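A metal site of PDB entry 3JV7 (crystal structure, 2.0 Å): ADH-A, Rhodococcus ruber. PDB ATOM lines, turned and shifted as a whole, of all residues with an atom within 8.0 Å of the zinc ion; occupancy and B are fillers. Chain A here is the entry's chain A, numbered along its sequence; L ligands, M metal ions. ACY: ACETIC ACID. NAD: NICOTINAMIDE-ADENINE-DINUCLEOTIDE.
OD2 of Asp 153 binds the zinc ion (1.9 Å). The zinc ion is bound by OXT of ACY L1. NE2 of His 62 is bound to the zinc ion (2.1 Å). The zinc ion is bound by the side-chain sulfur (SG) of Cys 38, at 2.3 Å.
The backbone NH of Trp 295 lies within hydrogen-bond range of an oxygen (O7N) of NAD L2 (2.7 Å). The guanidinium group (NH1) of Arg 340 lies within salt-bridge range of an oxygen (O1N) of NAD L2 (2.8 Å). The backbone NH (N) of Leu 183 is in hydrogen-bond range of an oxygen (O2N) of NAD L2, at 2.9 Å. An oxygen (O1N) of NAD L2 lies within hydrogen-bond range of the backbone NH (N) of His 39. An oxygen (O3D) of NAD L2 sits at hydrogen-bond distance from the backbone NH (N) of Ile 271 (3.0 Å). A ring nitrogen (ND1) of His 39 is in hydrogen-bond range of an oxygen (O1A) of NAD L2, 2.8 Å away. OG of Ser 40 is in hydrogen-bond range of O2D of NAD L2 (2.7 Å).
Residues that only touch the zinc ion: Ser 40 (3.9 Å). Of the 19 residues printed, 4 come within 4 Å of the zinc ion. The nearest printed residue that does not touch the zinc ion is Arg 340 (4.6 Å).
The side-chain carboxylate (OD1) of Asp 41 sits close to a ring nitrogen (ND1) of His 62 (3.3 Å). SG of Cys 38 sits close to NH2 of Arg 340 (3.5 Å). OG1 of Thr 157 is in hydrogen-bond range of OD1 of Asp 153 (2.8 Å). The backbone NH (N) of Cys 38 sits at hydrogen-bond distance from the side-chain carboxylate (OD2) of Asp 41, at 3.1 Å. SG of Cys 38 lies close to N of Ser 40, at 3.4 Å.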
ATOM      1  N   GLY A  36     -27.064  12.739  20.143  1.00  0.00           N
ATOM      2  CA  GLY A  36     -27.106  14.094  20.674  1.00  0.00           C
ATOM      3  C   GLY A  36     -28.374  14.849  20.321  1.00  0.00           C
ATOM      4  O   GLY A  36     -28.914  14.684  19.220  1.00  0.00           O
ATOM      5  N   LEU A  37     -28.867  15.646  21.261  1.00  0.00           N
ATOM      6  CA  LEU A  37     -29.972  16.577  21.009  1.00  0.00           C
ATOM      7  C   LEU A  37     -29.422  17.913  20.549  1.00  0.00           C
ATOM      8  O   LEU A  37     -28.501  18.447  21.157  1.00  0.00           O
ATOM      9  CB  LEU A  37     -30.796  16.809  22.275  1.00  0.00           C
ATOM     10  CG  LEU A  37     -31.720  15.677  22.728  1.00  0.00           C
ATOM     11  CD1 LEU A  37     -30.935  14.552  23.425  1.00  0.00           C
ATOM     12  CD2 LEU A  37     -32.810  16.222  23.646  1.00  0.00           C
ATOM     13  N   CYS A  38     -29.985  18.443  19.468  1.00  0.00           N
ATOM     14  CA  CYS A  38     -29.560  19.717  18.921  1.00  0.00           C
ATOM     15  C   CYS A  38     -30.719  20.696  18.948  1.00  0.00           C
ATOM     16  O   CYS A  38     -31.867  20.317  18.748  1.00  0.00           O
ATOM     17  CB  CYS A  38     -29.065  19.554  17.479  1.00  0.00           C
ATOM     18  SG  CYS A  38     -28.528  21.099  16.733  1.00  0.00           S
ATOM     19  N   HIS A  39     -30.432  21.974  19.181  1.00  0.00           N
ATOM     20  CA  HIS A  39     -31.502  22.965  19.188  1.00  0.00           C
ATOM     21  C   HIS A  39     -32.181  23.056  17.810  1.00  0.00           C
ATOM     22  O   HIS A  39     -33.311  23.558  17.714  1.00  0.00           O
ATOM     23  CB  HIS A  39     -30.971  24.331  19.640  1.00  0.00           C
ATOM     24  CG  HIS A  39     -32.052  25.244  20.151  1.00  0.00           C
ATOM     25  ND1 HIS A  39     -32.154  25.595  21.480  1.00  0.00           N
ATOM     26  CD2 HIS A  39     -33.075  25.858  19.524  1.00  0.00           C
ATOM     27  CE1 HIS A  39     -33.184  26.397  21.644  1.00  0.00           C
ATOM     28  NE2 HIS A  39     -33.770  26.571  20.476  1.00  0.00           N
ATOM     29  N   SER A  40     -31.533  22.594  16.760  1.00  0.00           N
ATOM     30  CA  SER A  40     -32.210  22.583  15.459  1.00  0.00           C
ATOM     31  C   SER A  40     -33.442  21.678  15.494  1.00  0.00           C
ATOM     32  O   SER A  40     -34.401  21.879  14.740  1.00  0.00           O
ATOM     33  CB  SER A  40     -31.278  22.185  14.311  1.00  0.00           C
ATOM     34  OG  SER A  40     -30.289  23.189  14.102  1.00  0.00           O
ATOM     35  N   ASP A  41     -33.425  20.699  16.385  1.00  0.00           N
ATOM     36  CA  ASP A  41     -34.565  19.795  16.559  1.00  0.00           C
ATOM     37  C   ASP A  41     -35.811  20.558  17.004  1.00  0.00           C
ATOM     38  O   ASP A  41     -36.928  20.265  16.562  1.00  0.00           O
ATOM     39  CB  ASP A  41     -34.215  18.713  17.581  1.00  0.00           C
ATOM     40  CG  ASP A  41     -33.123  17.789  17.078  1.00  0.00           C
ATOM     41  OD1 ASP A  41     -33.014  17.662  15.829  1.00  0.00           O
ATOM     42  OD2 ASP A  41     -32.385  17.211  17.897  1.00  0.00           O
ATOM     43  N   GLY A  61     -32.697  12.875  15.854  1.00  0.00           N
ATOM     44  CA  GLY A  61     -31.299  12.604  16.177  1.00  0.00           C
ATOM     45  C   GLY A  61     -30.368  12.689  14.981  1.00  0.00           C
ATOM     46  O   GLY A  61     -30.260  11.737  14.209  1.00  0.00           O
ATOM     47  N   HIS A  62     -29.684  13.817  14.814  1.00  0.00           N
ATOM     48  CA  HIS A  62     -28.717  13.952  13.725  1.00  0.00           C
ATOM     49  C   HIS A  62     -27.283  14.006  14.231  1.00  0.00           C
ATOM     50  O   HIS A  62     -26.352  14.208  13.454  1.00  0.00           O
ATOM     51  CB  HIS A  62     -29.055  15.109  12.762  1.00  0.00           C
ATOM     52  CG  HIS A  62     -29.194  16.446  13.434  1.00  0.00           C
ATOM     53  ND1 HIS A  62     -30.398  16.915  13.910  1.00  0.00           N
ATOM     54  CD2 HIS A  62     -28.304  17.446  13.639  1.00  0.00           C
ATOM     55  CE1 HIS A  62     -30.233  18.123  14.418  1.00  0.00           C
ATOM     56  NE2 HIS A  62     -28.973  18.469  14.259  1.00  0.00           N
ATOM     57  N   GLU A  63     -27.127  13.819  15.535  1.00  0.00           N
ATOM     58  CA  GLU A  63     -25.828  13.543  16.131  1.00  0.00           C
ATOM     59  C   GLU A  63     -25.803  12.087  16.576  1.00  0.00           C
ATOM     60  O   GLU A  63     -26.484  11.716  17.528  1.00  0.00           O
ATOM     61  CB  GLU A  63     -25.577  14.443  17.344  1.00  0.00           C
ATOM     62  CG  GLU A  63     -25.299  15.882  16.962  1.00  0.00           C
ATOM     63  CD  GLU A  63     -24.912  16.737  18.166  1.00  0.00           C
ATOM     64  OE1 GLU A  63     -25.215  16.319  19.317  1.00  0.00           O
ATOM     65  OE2 GLU A  63     -24.302  17.802  17.962  1.00  0.00           O
ATOM     66  N   LEU A 119     -33.154  14.406  10.060  1.00  0.00           N
ATOM     67  CA  LEU A 119     -33.645  15.602   9.368  1.00  0.00           C
ATOM     68  C   LEU A 119     -34.197  15.249   7.990  1.00  0.00           C
ATOM     69  O   LEU A 119     -33.932  15.935   7.006  1.00  0.00           O
ATOM     70  CB  LEU A 119     -32.533  16.676   9.267  1.00  0.00           C
ATOM     71  CG  LEU A 119     -31.916  17.164  10.590  1.00  0.00           C
ATOM     72  CD1 LEU A 119     -30.613  17.955  10.408  1.00  0.00           C
ATOM     73  CD2 LEU A 119     -32.925  17.988  11.372  1.00  0.00           C
ATOM     74  N   THR A 152     -20.251  15.387  16.152  1.00  0.00           N
ATOM     75  CA  THR A 152     -20.808  15.272  14.815  1.00  0.00           C
ATOM     76  C   THR A 152     -21.584  16.510  14.345  1.00  0.00           C
ATOM     77  O   THR A 152     -21.989  16.588  13.203  1.00  0.00           O
ATOM     78  CB  THR A 152     -21.723  14.037  14.680  1.00  0.00           C
ATOM     79  OG1 THR A 152     -22.818  14.155  15.593  1.00  0.00           O
ATOM     80  CG2 THR A 152     -20.952  12.752  14.963  1.00  0.00           C
ATOM     81  N   ASP A 153     -21.813  17.462  15.241  1.00  0.00           N
ATOM     82  CA  ASP A 153     -22.575  18.658  14.876  1.00  0.00           C
ATOM     83  C   ASP A 153     -22.172  19.829  15.768  1.00  0.00           C
ATOM     84  O   ASP A 153     -21.711  20.866  15.280  1.00  0.00           O
ATOM     85  CB  ASP A 153     -24.070  18.345  14.972  1.00  0.00           C
ATOM     86  CG  ASP A 153     -24.959  19.511  14.576  1.00  0.00           C
ATOM     87  OD1 ASP A 153     -24.450  20.577  14.131  1.00  0.00           O
ATOM     88  OD2 ASP A 153     -26.188  19.349  14.738  1.00  0.00           O
ATOM     89  N   ALA A 154     -22.310  19.660  17.090  1.00  0.00           N
ATOM     90  CA  ALA A 154     -21.841  20.671  18.021  1.00  0.00           C
ATOM     91  C   ALA A 154     -20.342  20.945  17.838  1.00  0.00           C
ATOM     92  O   ALA A 154     -19.864  22.042  18.134  1.00  0.00           O
ATOM     93  CB  ALA A 154     -22.162  20.252  19.474  1.00  0.00           C
ATOM     94  N   THR A 157     -20.060  21.721  13.204  1.00  0.00           N
ATOM     95  CA  THR A 157     -20.607  22.969  12.691  1.00  0.00           C
ATOM     96  C   THR A 157     -19.773  24.219  13.031  1.00  0.00           C
ATOM     97  O   THR A 157     -19.393  24.967  12.123  1.00  0.00           O
ATOM     98  CB  THR A 157     -22.098  23.100  13.037  1.00  0.00           C
ATOM     99  OG1 THR A 157     -22.798  22.002  12.422  1.00  0.00           O
ATOM    100  CG2 THR A 157     -22.662  24.417  12.523  1.00  0.00           C
ATOM    101  N   LEU A 183     -23.257  24.078  20.730  1.00  0.00           N
ATOM    102  CA  LEU A 183     -22.268  24.477  19.726  1.00  0.00           C
ATOM    103  C   LEU A 183     -21.244  25.464  20.290  1.00  0.00           C
ATOM    104  O   LEU A 183     -20.052  25.313  20.088  1.00  0.00           O
ATOM    105  CB  LEU A 183     -22.947  25.146  18.504  1.00  0.00           C
ATOM    106  CG  LEU A 183     -23.369  24.243  17.324  1.00  0.00           C
ATOM    107  CD1 LEU A 183     -24.495  23.308  17.747  1.00  0.00           C
ATOM    108  CD2 LEU A 183     -23.793  25.068  16.118  1.00  0.00           C
ATOM    109  N   ILE A 271     -30.002  29.682  14.088  1.00  0.00           N
ATOM    110  CA  ILE A 271     -31.141  29.762  13.191  1.00  0.00           C
ATOM    111  C   ILE A 271     -32.386  30.341  13.874  1.00  0.00           C
ATOM    112  O   ILE A 271     -32.950  29.715  14.780  1.00  0.00           O
ATOM    113  CB  ILE A 271     -31.479  28.382  12.623  1.00  0.00           C
ATOM    114  CG1 ILE A 271     -30.266  27.821  11.852  1.00  0.00           C
ATOM    115  CG2 ILE A 271     -32.718  28.459  11.737  1.00  0.00           C
ATOM    116  CD1 ILE A 271     -30.404  26.355  11.472  1.00  0.00           C
ATOM    117  N   TYR A 294     -23.337  25.919   6.700  1.00  0.00           N
ATOM    118  CA  TYR A 294     -24.156  24.740   6.984  1.00  0.00           C
ATOM    119  C   TYR A 294     -23.313  23.537   7.397  1.00  0.00           C
ATOM    120  O   TYR A 294     -22.500  23.047   6.612  1.00  0.00           O
ATOM    121  CB  TYR A 294     -24.999  24.395   5.774  1.00  0.00           C
ATOM    122  CG  TYR A 294     -25.796  23.099   5.891  1.00  0.00           C
ATOM    123  CD1 TYR A 294     -26.676  22.897   6.939  1.00  0.00           C
ATOM    124  CD2 TYR A 294     -25.696  22.113   4.913  1.00  0.00           C
ATOM    125  CE1 TYR A 294     -27.427  21.731   7.032  1.00  0.00           C
ATOM    126  CE2 TYR A 294     -26.435  20.939   4.995  1.00  0.00           C
ATOM    127  CZ  TYR A 294     -27.296  20.748   6.054  1.00  0.00           C
ATOM    128  OH  TYR A 294     -28.048  19.593   6.138  1.00  0.00           O
ATOM    129  N   TRP A 295     -23.481  23.081   8.631  1.00  0.00           N
ATOM    130  CA  TRP A 295     -22.845  21.842   9.073  1.00  0.00           C
ATOM    131  C   TRP A 295     -21.348  21.850   8.755  1.00  0.00           C
ATOM    132  O   TRP A 295     -20.666  22.826   9.052  1.00  0.00           O
ATOM    133  CB  TRP A 295     -23.572  20.617   8.482  1.00  0.00           C
ATOM    134  CG  TRP A 295     -23.803  19.515   9.492  1.00  0.00           C
ATOM    135  CD1 TRP A 295     -23.002  19.206  10.547  1.00  0.00           C
ATOM    136  CD2 TRP A 295     -24.902  18.594   9.523  1.00  0.00           C
ATOM    137  NE1 TRP A 295     -23.530  18.144  11.255  1.00  0.00           N
ATOM    138  CE2 TRP A 295     -24.697  17.746  10.649  1.00  0.00           C
ATOM    139  CE3 TRP A 295     -26.030  18.397   8.730  1.00  0.00           C
ATOM    140  CZ2 TRP A 295     -25.582  16.716  10.984  1.00  0.00           C
ATOM    141  CZ3 TRP A 295     -26.925  17.366   9.065  1.00  0.00           C
ATOM    142  CH2 TRP A 295     -26.683  16.543  10.184  1.00  0.00           C
ATOM    143  N   ARG A 340     -24.443  19.812  26.105  1.00  0.00           N
ATOM    144  CA  ARG A 340     -25.191  18.963  25.180  1.00  0.00           C
ATOM    145  C   ARG A 340     -25.955  17.846  25.885  1.00  0.00           C
ATOM    146  O   ARG A 340     -25.391  17.116  26.707  1.00  0.00           O
ATOM    147  CB  ARG A 340     -24.243  18.334  24.173  1.00  0.00           C
ATOM    148  CG  ARG A 340     -24.265  18.961  22.793  1.00  0.00           C
ATOM    149  CD  ARG A 340     -25.536  18.588  22.071  1.00  0.00           C
ATOM    150  NE  ARG A 340     -25.452  18.888  20.636  1.00  0.00           N
ATOM    151  CZ  ARG A 340     -25.924  19.998  20.073  1.00  0.00           C
ATOM    152  NH1 ARG A 340     -26.505  20.946  20.802  1.00  0.00           N
ATOM    153  NH2 ARG A 340     -25.806  20.165  18.761  1.00  0.00           N
HETATM  154  C   ACY L   1     -28.360  21.326  12.019  1.00  0.00           C
HETATM  155  O   ACY L   1     -29.119  21.918  11.232  1.00  0.00           O
HETATM  156  OXT ACY L   1     -28.409  21.461  13.258  1.00  0.00           O
HETATM  157  CH3 ACY L   1     -27.330  20.419  11.418  1.00  0.00           C
HETATM  158  PA  NAD L   2     -28.474  25.360  22.736  1.00  0.00           P
HETATM  159  O1A NAD L   2     -29.911  25.363  23.104  1.00  0.00           O
HETATM  160  O2A NAD L   2     -27.667  24.217  23.207  1.00  0.00           O
HETATM  161  O5B NAD L   2     -27.775  26.664  23.327  1.00  0.00           O
HETATM  162  C5B NAD L   2     -28.354  27.946  23.222  1.00  0.00           C
HETATM  163  C4B NAD L   2     -27.458  28.911  23.998  1.00  0.00           C
HETATM  164  O4B NAD L   2     -27.657  30.191  23.443  1.00  0.00           O
HETATM  165  C3B NAD L   2     -27.835  29.010  25.481  1.00  0.00           C
HETATM  166  O3B NAD L   2     -26.667  29.119  26.271  1.00  0.00           O
HETATM  167  C2B NAD L   2     -28.588  30.330  25.555  1.00  0.00           C
HETATM  168  O2B NAD L   2     -28.412  30.989  26.768  1.00  0.00           O
HETATM  169  C1B NAD L   2     -27.901  31.115  24.466  1.00  0.00           C
HETATM  170  N9A NAD L   2     -28.697  32.244  23.962  1.00  0.00           N
HETATM  171  C8A NAD L   2     -30.013  32.219  23.558  1.00  0.00           C
HETATM  172  N7A NAD L   2     -30.348  33.462  23.172  1.00  0.00           N
HETATM  173  C5A NAD L   2     -29.267  34.278  23.310  1.00  0.00           C
HETATM  174  C6A NAD L   2     -29.089  35.620  23.048  1.00  0.00           C
HETATM  175  N6A NAD L   2     -30.135  36.366  22.710  1.00  0.00           N
HETATM  176  N1A NAD L   2     -27.851  36.187  23.272  1.00  0.00           N
HETATM  177  C2A NAD L   2     -26.822  35.419  23.768  1.00  0.00           C
HETATM  178  N3A NAD L   2     -27.012  34.086  24.031  1.00  0.00           N
HETATM  179  C4A NAD L   2     -28.230  33.521  23.807  1.00  0.00           C
HETATM  180  O3  NAD L   2     -28.415  25.500  21.119  1.00  0.00           O
HETATM  181  PN  NAD L   2     -27.416  24.677  20.166  1.00  0.00           P
HETATM  182  O1N NAD L   2     -27.870  23.268  20.101  1.00  0.00           O
HETATM  183  O2N NAD L   2     -26.020  24.990  20.525  1.00  0.00           O
HETATM  184  O5D NAD L   2     -27.781  25.409  18.786  1.00  0.00           O
HETATM  185  C5D NAD L   2     -27.567  26.798  18.661  1.00  0.00           C
HETATM  186  C4D NAD L   2     -28.126  27.281  17.322  1.00  0.00           C
HETATM  187  O4D NAD L   2     -27.339  26.743  16.269  1.00  0.00           O
HETATM  188  C3D NAD L   2     -29.555  26.811  17.054  1.00  0.00           C
HETATM  189  O3D NAD L   2     -30.274  27.879  16.460  1.00  0.00           O
HETATM  190  C2D NAD L   2     -29.393  25.716  16.030  1.00  0.00           C
HETATM  191  O2D NAD L   2     -30.507  25.660  15.185  1.00  0.00           O
HETATM  192  C1D NAD L   2     -28.197  26.260  15.253  1.00  0.00           C
HETATM  193  N1N NAD L   2     -27.452  25.276  14.466  1.00  0.00           N
HETATM  194  C2N NAD L   2     -27.101  25.615  13.182  1.00  0.00           C
HETATM  195  C3N NAD L   2     -26.356  24.730  12.418  1.00  0.00           C
HETATM  196  C7N NAD L   2     -25.929  25.112  11.028  1.00  0.00           C
HETATM  197  O7N NAD L   2     -25.376  24.133  10.204  1.00  0.00           O
HETATM  198  N7N NAD L   2     -26.054  26.369  10.630  1.00  0.00           N
HETATM  199  C4N NAD L   2     -25.962  23.502  12.967  1.00  0.00           C
HETATM  200  C5N NAD L   2     -26.314  23.171  14.271  1.00  0.00           C
HETATM  201  C6N NAD L   2     -27.061  24.078  15.018  1.00  0.00           C
HETATM  202 ZN    ZN M   1     -27.919  20.207  14.689  1.00  0.00          ZN
